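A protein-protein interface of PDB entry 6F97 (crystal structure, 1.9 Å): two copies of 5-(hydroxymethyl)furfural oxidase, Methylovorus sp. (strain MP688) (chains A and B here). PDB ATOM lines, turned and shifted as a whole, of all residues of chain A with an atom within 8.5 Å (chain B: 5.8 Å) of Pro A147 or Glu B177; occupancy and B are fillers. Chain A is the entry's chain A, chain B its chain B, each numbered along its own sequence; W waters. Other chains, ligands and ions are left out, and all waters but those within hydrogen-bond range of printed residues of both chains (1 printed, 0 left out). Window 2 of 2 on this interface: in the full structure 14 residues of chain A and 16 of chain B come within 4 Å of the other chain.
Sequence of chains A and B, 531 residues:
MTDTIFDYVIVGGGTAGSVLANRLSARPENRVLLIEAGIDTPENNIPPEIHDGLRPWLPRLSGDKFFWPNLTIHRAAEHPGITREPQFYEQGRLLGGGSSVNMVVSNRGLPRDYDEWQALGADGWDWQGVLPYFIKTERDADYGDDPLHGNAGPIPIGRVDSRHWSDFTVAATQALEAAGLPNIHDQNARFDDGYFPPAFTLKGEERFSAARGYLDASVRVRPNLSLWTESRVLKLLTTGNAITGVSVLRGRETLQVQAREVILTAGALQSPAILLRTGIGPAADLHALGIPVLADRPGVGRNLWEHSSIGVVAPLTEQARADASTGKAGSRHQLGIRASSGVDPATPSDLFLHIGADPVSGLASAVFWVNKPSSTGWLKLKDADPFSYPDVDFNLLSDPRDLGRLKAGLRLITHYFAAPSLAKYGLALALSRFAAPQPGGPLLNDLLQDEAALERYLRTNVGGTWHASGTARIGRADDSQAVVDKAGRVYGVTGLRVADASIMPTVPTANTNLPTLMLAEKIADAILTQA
Among the printed residues, pairs that only touch across the chains: Gln A128 with Ala B179, Leu A131 with Gly B180 and Pro A147 with Glu B177.
NE2 of Gln A128 lies within hydrogen-bond range of O of Ala B178, at 3.3 Å.
The backbone carbonyl oxygen (O) of Gly B180 sits at hydrogen-bond distance from the indole nitrogen (NE1) of Trp A127 (3.0 Å).
No position is printed for both chains.
Water W1 bridges O of Gln A128 and O of Ala B178.
Of the 17 printed residues of chain A, 4 touch a printed residue of chain B.
Among the printed residues, 5 pairs touch across the chains.
Among the printed residues, no Asp or Glu carboxylate lies within 4 Å of a Lys or Arg side-chain nitrogen of the other chain.
Of the printed residues of chain B, Trp A127 touches Gly B180.
Of the printed residues of chain B, Gln A128 touches Ala B178 (3.3 Å) and Ala B179 (3.5 Å).
Asp A145 touches none of the printed residues of chain B.
Pro A147 touches just one residue of chain B: Glu B177 (3.7 Å).
Glu B177 touches just one residue of chain A: Pro A147.
Of the printed residues of chain A, Ala B178 touches Gln A128 (3.3 Å).
Printed residues of chain A within 4 Å of Ala B179: Gln A128 (3.5 Å).
Of the printed residues of chain A, Gly B180 touches Trp A127 and Leu A131.
The nearest residue of chain B that does not touch Pro A147 is Tyr B195 (5.6 Å).
The nearest residue of chain A that does not touch Glu B177 is Leu A131 (4.6 Å).
The nearest printed residue of chain B that does not touch Leu A131 is Glu B177 (4.6 Å).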
ATOM      1  N   ARG A 108     -15.439 -36.796 -17.652  1.00  0.00           N
ATOM      2  CA  ARG A 108     -15.642 -36.062 -16.379  1.00  0.00           C
ATOM      3  C   ARG A 108     -16.240 -36.893 -15.262  1.00  0.00           C
ATOM      4  O   ARG A 108     -16.082 -36.593 -14.052  1.00  0.00           O
ATOM      5  CB  ARG A 108     -16.509 -34.784 -16.637  1.00  0.00           C
ATOM      6  CG  ARG A 108     -16.216 -34.122 -17.970  1.00  0.00           C
ATOM      7  CD  ARG A 108     -16.043 -32.626 -18.060  1.00  0.00           C
ATOM      8  NE  ARG A 108     -17.288 -32.014 -18.259  1.00  0.00           N
ATOM      9  CZ  ARG A 108     -17.591 -30.855 -18.850  1.00  0.00           C
ATOM     10  NH1 ARG A 108     -16.751 -29.943 -19.301  1.00  0.00           N
ATOM     11  NH2 ARG A 108     -18.869 -30.585 -18.902  1.00  0.00           N
ATOM     12  N   TRP A 127     -21.213 -30.871  -7.956  1.00  0.00           N
ATOM     13  CA  TRP A 127     -21.202 -30.707  -9.374  1.00  0.00           C
ATOM     14  C   TRP A 127     -21.227 -29.274  -9.801  1.00  0.00           C
ATOM     15  O   TRP A 127     -20.462 -28.854 -10.715  1.00  0.00           O
ATOM     16  CB  TRP A 127     -22.377 -31.483 -10.015  1.00  0.00           C
ATOM     17  CG  TRP A 127     -22.500 -31.302 -11.485  1.00  0.00           C
ATOM     18  CD1 TRP A 127     -23.544 -30.767 -12.134  1.00  0.00           C
ATOM     19  CD2 TRP A 127     -21.550 -31.684 -12.496  1.00  0.00           C
ATOM     20  NE1 TRP A 127     -23.316 -30.731 -13.486  1.00  0.00           N
ATOM     21  CE2 TRP A 127     -22.116 -31.320 -13.752  1.00  0.00           C
ATOM     22  CE3 TRP A 127     -20.286 -32.298 -12.473  1.00  0.00           C
ATOM     23  CZ2 TRP A 127     -21.476 -31.573 -14.978  1.00  0.00           C
ATOM     24  CZ3 TRP A 127     -19.634 -32.547 -13.720  1.00  0.00           C
ATOM     25  CH2 TRP A 127     -20.218 -32.185 -14.924  1.00  0.00           C
ATOM     26  N   GLN A 128     -22.132 -28.513  -9.197  1.00  0.00           N
ATOM     27  CA  GLN A 128     -22.187 -27.066  -9.455  1.00  0.00           C
ATOM     28  C   GLN A 128     -20.842 -26.378  -9.212  1.00  0.00           C
ATOM     29  O   GLN A 128     -20.465 -25.480  -9.975  1.00  0.00           O
ATOM     30  CB  GLN A 128     -23.274 -26.397  -8.580  1.00  0.00           C
ATOM     31  CG  GLN A 128     -23.152 -24.883  -8.443  1.00  0.00           C
ATOM     32  CD  GLN A 128     -24.398 -24.255  -7.852  1.00  0.00           C
ATOM     33  OE1 GLN A 128     -25.190 -24.931  -7.206  1.00  0.00           O
ATOM     34  NE2 GLN A 128     -24.595 -22.982  -8.126  1.00  0.00           N
ATOM     35  N   LEU A 131     -17.949 -28.075 -11.904  1.00  0.00           N
ATOM     36  CA  LEU A 131     -18.246 -27.753 -13.315  1.00  0.00           C
ATOM     37  C   LEU A 131     -17.468 -26.562 -13.937  1.00  0.00           C
ATOM     38  O   LEU A 131     -16.872 -26.737 -14.985  1.00  0.00           O
ATOM     39  CB  LEU A 131     -19.765 -27.617 -13.563  1.00  0.00           C
ATOM     40  CG  LEU A 131     -20.154 -27.244 -15.005  1.00  0.00           C
ATOM     41  CD1 LEU A 131     -19.630 -28.255 -16.034  1.00  0.00           C
ATOM     42  CD2 LEU A 131     -21.669 -27.063 -15.122  1.00  0.00           C
ATOM     43  N   PRO A 132     -17.443 -25.374 -13.288  1.00  0.00           N
ATOM     44  CA  PRO A 132     -16.584 -24.242 -13.806  1.00  0.00           C
ATOM     45  C   PRO A 132     -15.105 -24.636 -14.053  1.00  0.00           C
ATOM     46  O   PRO A 132     -14.510 -24.188 -15.000  1.00  0.00           O
ATOM     47  CB  PRO A 132     -16.676 -23.167 -12.705  1.00  0.00           C
ATOM     48  CG  PRO A 132     -17.914 -23.495 -11.924  1.00  0.00           C
ATOM     49  CD  PRO A 132     -18.251 -24.978 -12.126  1.00  0.00           C
ATOM     50  N   ILE A 135     -14.829 -26.784 -17.251  1.00  0.00           N
ATOM     51  CA  ILE A 135     -14.969 -25.877 -18.400  1.00  0.00           C
ATOM     52  C   ILE A 135     -13.626 -25.169 -18.610  1.00  0.00           C
ATOM     53  O   ILE A 135     -13.161 -25.112 -19.732  1.00  0.00           O
ATOM     54  CB  ILE A 135     -16.128 -24.851 -18.239  1.00  0.00           C
ATOM     55  CG1 ILE A 135     -17.503 -25.563 -18.402  1.00  0.00           C
ATOM     56  CG2 ILE A 135     -16.091 -23.704 -19.276  1.00  0.00           C
ATOM     57  CD1 ILE A 135     -18.693 -24.832 -17.746  1.00  0.00           C
ATOM     58  N   GLU A 138     -10.707 -27.196 -20.479  1.00  0.00           N
ATOM     59  CA  GLU A 138     -10.861 -27.768 -21.796  1.00  0.00           C
ATOM     60  C   GLU A 138     -11.095 -26.741 -22.891  1.00  0.00           C
ATOM     61  O   GLU A 138     -11.605 -25.625 -22.654  1.00  0.00           O
ATOM     62  CB  GLU A 138     -12.011 -28.742 -21.791  1.00  0.00           C
ATOM     63  CG  GLU A 138     -13.377 -28.045 -21.798  1.00  0.00           C
ATOM     64  CD  GLU A 138     -14.598 -28.984 -21.863  1.00  0.00           C
ATOM     65  OE1 GLU A 138     -14.471 -30.187 -21.614  1.00  0.00           O
ATOM     66  OE2 GLU A 138     -15.681 -28.469 -22.168  1.00  0.00           O
ATOM     67  N   TYR A 143     -18.117 -29.381 -29.160  1.00  0.00           N
ATOM     68  CA  TYR A 143     -19.193 -28.738 -28.404  1.00  0.00           C
ATOM     69  C   TYR A 143     -18.765 -27.586 -27.516  1.00  0.00           C
ATOM     70  O   TYR A 143     -19.494 -27.203 -26.604  1.00  0.00           O
ATOM     71  CB  TYR A 143     -19.861 -29.772 -27.499  1.00  0.00           C
ATOM     72  CG  TYR A 143     -20.295 -30.990 -28.243  1.00  0.00           C
ATOM     73  CD1 TYR A 143     -19.711 -32.243 -28.010  1.00  0.00           C
ATOM     74  CD2 TYR A 143     -21.289 -30.907 -29.179  1.00  0.00           C
ATOM     75  CE1 TYR A 143     -20.116 -33.363 -28.719  1.00  0.00           C
ATOM     76  CE2 TYR A 143     -21.712 -32.018 -29.892  1.00  0.00           C
ATOM     77  CZ  TYR A 143     -21.136 -33.237 -29.669  1.00  0.00           C
ATOM     78  OH  TYR A 143     -21.606 -34.314 -30.375  1.00  0.00           O
ATOM     79  N   GLY A 144     -17.618 -27.006 -27.793  1.00  0.00           N
ATOM     80  CA  GLY A 144     -17.037 -25.934 -26.978  1.00  0.00           C
ATOM     81  C   GLY A 144     -17.875 -24.678 -26.801  1.00  0.00           C
ATOM     82  O   GLY A 144     -17.679 -23.944 -25.812  1.00  0.00           O
ATOM     83  N   ASP A 145     -18.800 -24.434 -27.745  1.00  0.00           N
ATOM     84  CA  ASP A 145     -19.764 -23.326 -27.662  1.00  0.00           C
ATOM     85  C   ASP A 145     -20.944 -23.570 -26.728  1.00  0.00           C
ATOM     86  O   ASP A 145     -21.628 -22.616 -26.346  1.00  0.00           O
ATOM     87  CB  ASP A 145     -20.361 -23.029 -29.047  1.00  0.00           C
ATOM     88  CG  ASP A 145     -19.341 -22.489 -30.044  1.00  0.00           C
ATOM     89  OD1 ASP A 145     -18.254 -22.015 -29.618  1.00  0.00           O
ATOM     90  OD2 ASP A 145     -19.661 -22.539 -31.263  1.00  0.00           O
ATOM     91  N   ASP A 146     -21.204 -24.828 -26.387  1.00  0.00           N
ATOM     92  CA  ASP A 146     -22.415 -25.191 -25.650  1.00  0.00           C
ATOM     93  C   ASP A 146     -22.231 -24.895 -24.117  1.00  0.00           C
ATOM     94  O   ASP A 146     -21.095 -24.739 -23.647  1.00  0.00           O
ATOM     95  CB  ASP A 146     -22.817 -26.657 -25.922  1.00  0.00           C
ATOM     96  CG  ASP A 146     -23.003 -26.992 -27.418  1.00  0.00           C
ATOM     97  OD1 ASP A 146     -22.633 -26.181 -28.305  1.00  0.00           O
ATOM     98  OD2 ASP A 146     -23.511 -28.117 -27.685  1.00  0.00           O
ATOM     99  N   PRO A 147     -23.351 -24.824 -23.348  1.00  0.00           N
ATOM    100  CA  PRO A 147     -23.401 -24.368 -21.928  1.00  0.00           C
ATOM    101  C   PRO A 147     -22.483 -25.045 -20.865  1.00  0.00           C
ATOM    102  O   PRO A 147     -21.961 -24.365 -19.926  1.00  0.00           O
ATOM    103  CB  PRO A 147     -24.862 -24.637 -21.542  1.00  0.00           C
ATOM    104  CG  PRO A 147     -25.616 -24.581 -22.826  1.00  0.00           C
ATOM    105  CD  PRO A 147     -24.707 -25.165 -23.850  1.00  0.00           C
ATOM    106  N   LEU A 148     -22.368 -26.359 -20.967  1.00  0.00           N
ATOM    107  CA  LEU A 148     -21.564 -27.176 -20.035  1.00  0.00           C
ATOM    108  C   LEU A 148     -20.125 -27.396 -20.510  1.00  0.00           C
ATOM    109  O   LEU A 148     -19.408 -28.225 -19.930  1.00  0.00           O
ATOM    110  CB  LEU A 148     -22.227 -28.545 -19.810  1.00  0.00           C
ATOM    111  CG  LEU A 148     -23.292 -28.592 -18.741  1.00  0.00           C
ATOM    112  CD1 LEU A 148     -24.349 -27.511 -18.877  1.00  0.00           C
ATOM    113  CD2 LEU A 148     -23.938 -29.973 -18.773  1.00  0.00           C
ATOM    114  N   HIS A 149     -19.691 -26.641 -21.517  1.00  0.00           N
ATOM    115  CA  HIS A 149     -18.354 -26.775 -22.081  1.00  0.00           C
ATOM    116  C   HIS A 149     -17.576 -25.459 -22.143  1.00  0.00           C
ATOM    117  O   HIS A 149     -18.109 -24.346 -21.974  1.00  0.00           O
ATOM    118  CB  HIS A 149     -18.423 -27.358 -23.493  1.00  0.00           C
ATOM    119  CG  HIS A 149     -18.787 -28.814 -23.546  1.00  0.00           C
ATOM    120  ND1 HIS A 149     -17.937 -29.812 -23.124  1.00  0.00           N
ATOM    121  CD2 HIS A 149     -19.881 -29.436 -24.053  1.00  0.00           C
ATOM    122  CE1 HIS A 149     -18.501 -30.983 -23.359  1.00  0.00           C
ATOM    123  NE2 HIS A 149     -19.679 -30.785 -23.932  1.00  0.00           N
ATOM    124  N   GLY A 150     -16.294 -25.627 -22.394  1.00  0.00           N
ATOM    125  CA  GLY A 150     -15.397 -24.535 -22.651  1.00  0.00           C
ATOM    126  C   GLY A 150     -14.777 -24.672 -24.005  1.00  0.00           C
ATOM    127  O   GLY A 150     -14.670 -25.789 -24.560  1.00  0.00           O
ATOM    128  N   ASP A 186     -22.280 -37.041 -26.486  1.00  0.00           N
ATOM    129  CA  ASP A 186     -21.349 -36.248 -25.723  1.00  0.00           C
ATOM    130  C   ASP A 186     -21.383 -36.749 -24.301  1.00  0.00           C
ATOM    131  O   ASP A 186     -22.217 -36.304 -23.514  1.00  0.00           O
ATOM    132  CB  ASP A 186     -21.725 -34.757 -25.793  1.00  0.00           C
ATOM    133  CG  ASP A 186     -20.778 -33.883 -24.985  1.00  0.00           C
ATOM    134  OD1 ASP A 186     -19.842 -34.440 -24.420  1.00  0.00           O
ATOM    135  OD2 ASP A 186     -20.939 -32.663 -24.919  1.00  0.00           O
ATOM    136  N   ALA A 189     -21.365 -33.906 -21.351  1.00  0.00           N
ATOM    137  CA  ALA A 189     -22.475 -32.999 -20.978  1.00  0.00           C
ATOM    138  C   ALA A 189     -23.841 -33.702 -20.895  1.00  0.00           C
ATOM    139  O   ALA A 189     -24.863 -33.015 -20.778  1.00  0.00           O
ATOM    140  CB  ALA A 189     -22.568 -31.820 -21.943  1.00  0.00           C
ATOM    141  N   ALA B 172     -34.897 -18.451 -15.838  1.00  0.00           N
ATOM    142  CA  ALA B 172     -34.957 -19.716 -15.060  1.00  0.00           C
ATOM    143  C   ALA B 172     -33.912 -20.717 -15.556  1.00  0.00           C
ATOM    144  O   ALA B 172     -33.146 -21.287 -14.767  1.00  0.00           O
ATOM    145  CB  ALA B 172     -36.330 -20.318 -15.112  1.00  0.00           C
ATOM    146  N   THR B 173     -33.838 -20.855 -16.866  1.00  0.00           N
ATOM    147  CA  THR B 173     -32.845 -21.739 -17.476  1.00  0.00           C
ATOM    148  C   THR B 173     -31.405 -21.323 -17.136  1.00  0.00           C
ATOM    149  O   THR B 173     -30.551 -22.199 -16.889  1.00  0.00           O
ATOM    150  CB  THR B 173     -33.034 -21.931 -18.996  1.00  0.00           C
ATOM    151  OG1 THR B 173     -32.858 -20.703 -19.711  1.00  0.00           O
ATOM    152  CG2 THR B 173     -34.382 -22.510 -19.270  1.00  0.00           C
ATOM    153  N   GLN B 174     -31.149 -20.018 -17.035  1.00  0.00           N
ATOM    154  CA  GLN B 174     -29.813 -19.551 -16.620  1.00  0.00           C
ATOM    155  C   GLN B 174     -29.507 -19.912 -15.199  1.00  0.00           C
ATOM    156  O   GLN B 174     -28.383 -20.230 -14.890  1.00  0.00           O
ATOM    157  CB  GLN B 174     -29.648 -18.061 -16.814  1.00  0.00           C
ATOM    158  CG  GLN B 174     -29.758 -17.655 -18.274  1.00  0.00           C
ATOM    159  CD  GLN B 174     -29.653 -16.151 -18.459  1.00  0.00           C
ATOM    160  OE1 GLN B 174     -29.787 -15.369 -17.506  1.00  0.00           O
ATOM    161  NE2 GLN B 174     -29.402 -15.736 -19.687  1.00  0.00           N
ATOM    162  N   ALA B 175     -30.499 -19.901 -14.324  1.00  0.00           N
ATOM    163  CA  ALA B 175     -30.276 -20.361 -12.952  1.00  0.00           C
ATOM    164  C   ALA B 175     -30.034 -21.881 -12.909  1.00  0.00           C
ATOM    165  O   ALA B 175     -29.275 -22.368 -12.120  1.00  0.00           O
ATOM    166  CB  ALA B 175     -31.459 -20.037 -12.098  1.00  0.00           C
ATOM    167  N   LEU B 176     -30.743 -22.622 -13.732  1.00  0.00           N
ATOM    168  CA  LEU B 176     -30.589 -24.073 -13.754  1.00  0.00           C
ATOM    169  C   LEU B 176     -29.210 -24.442 -14.326  1.00  0.00           C
ATOM    170  O   LEU B 176     -28.529 -25.297 -13.781  1.00  0.00           O
ATOM    171  CB  LEU B 176     -31.730 -24.706 -14.557  1.00  0.00           C
ATOM    172  CG  LEU B 176     -33.135 -24.446 -13.938  1.00  0.00           C
ATOM    173  CD1 LEU B 176     -34.236 -25.052 -14.790  1.00  0.00           C
ATOM    174  CD2 LEU B 176     -33.241 -24.999 -12.534  1.00  0.00           C
ATOM    175  N   GLU B 177     -28.814 -23.756 -15.397  1.00  0.00           N
ATOM    176  CA  GLU B 177     -27.472 -23.864 -15.957  1.00  0.00           C
ATOM    177  C   GLU B 177     -26.371 -23.695 -14.921  1.00  0.00           C
ATOM    178  O   GLU B 177     -25.457 -24.535 -14.852  1.00  0.00           O
ATOM    179  CB  GLU B 177     -27.231 -22.800 -17.002  1.00  0.00           C
ATOM    180  CG  GLU B 177     -27.693 -23.152 -18.388  1.00  0.00           C
ATOM    181  CD  GLU B 177     -26.982 -22.334 -19.452  1.00  0.00           C
ATOM    182  OE1 GLU B 177     -25.889 -21.776 -19.174  1.00  0.00           O
ATOM    183  OE2 GLU B 177     -27.514 -22.269 -20.576  1.00  0.00           O
ATOM    184  N   ALA B 178     -26.466 -22.613 -14.137  1.00  0.00           N
ATOM    185  CA  ALA B 178     -25.495 -22.296 -13.063  1.00  0.00           C
ATOM    186  C   ALA B 178     -25.411 -23.379 -11.988  1.00  0.00           C
ATOM    187  O   ALA B 178     -24.366 -23.554 -11.365  1.00  0.00           O
ATOM    188  CB  ALA B 178     -25.804 -20.946 -12.430  1.00  0.00           C
ATOM    189  N   ALA B 179     -26.492 -24.122 -11.764  1.00  0.00           N
ATOM    190  CA  ALA B 179     -26.423 -25.288 -10.865  1.00  0.00           C
ATOM    191  C   ALA B 179     -25.824 -26.531 -11.571  1.00  0.00           C
ATOM    192  O   ALA B 179     -25.633 -27.556 -10.929  1.00  0.00           O
ATOM    193  CB  ALA B 179     -27.812 -25.604 -10.297  1.00  0.00           C
ATOM    194  N   GLY B 180     -25.592 -26.463 -12.886  1.00  0.00           N
ATOM    195  CA  GLY B 180     -24.991 -27.582 -13.661  1.00  0.00           C
ATOM    196  C   GLY B 180     -25.956 -28.449 -14.463  1.00  0.00           C
ATOM    197  O   GLY B 180     -25.537 -29.438 -15.043  1.00  0.00           O
ATOM    198  N   LEU B 181     -27.229 -28.059 -14.517  1.00  0.00           N
ATOM    199  CA  LEU B 181     -28.259 -28.761 -15.258  1.00  0.00           C
ATOM    200  C   LEU B 181     -28.228 -28.467 -16.740  1.00  0.00           C
ATOM    201  O   LEU B 181     -28.265 -27.323 -17.161  1.00  0.00           O
ATOM    202  CB  LEU B 181     -29.654 -28.411 -14.715  1.00  0.00           C
ATOM    203  CG  LEU B 181     -29.837 -28.898 -13.267  1.00  0.00           C
ATOM    204  CD1 LEU B 181     -31.181 -28.412 -12.745  1.00  0.00           C
ATOM    205  CD2 LEU B 181     -29.772 -30.426 -13.192  1.00  0.00           C
ATOM    206  N   TYR B 195     -33.411 -29.883 -17.515  1.00  0.00           N
ATOM    207  CA  TYR B 195     -34.593 -29.131 -17.792  1.00  0.00           C
ATOM    208  C   TYR B 195     -34.879 -29.248 -19.268  1.00  0.00           C
ATOM    209  O   TYR B 195     -34.013 -29.653 -20.061  1.00  0.00           O
ATOM    210  CB  TYR B 195     -34.458 -27.650 -17.318  1.00  0.00           C
ATOM    211  CG  TYR B 195     -33.421 -26.821 -18.064  1.00  0.00           C
ATOM    212  CD1 TYR B 195     -32.117 -26.662 -17.538  1.00  0.00           C
ATOM    213  CD2 TYR B 195     -33.708 -26.244 -19.275  1.00  0.00           C
ATOM    214  CE1 TYR B 195     -31.151 -25.912 -18.188  1.00  0.00           C
ATOM    215  CE2 TYR B 195     -32.711 -25.493 -19.949  1.00  0.00           C
ATOM    216  CZ  TYR B 195     -31.466 -25.347 -19.381  1.00  0.00           C
ATOM    217  OH  TYR B 195     -30.502 -24.680 -20.014  1.00  0.00           O
HETATM  218  O   HOH W   1     -21.542 -24.183 -12.027  1.00  0.00           O
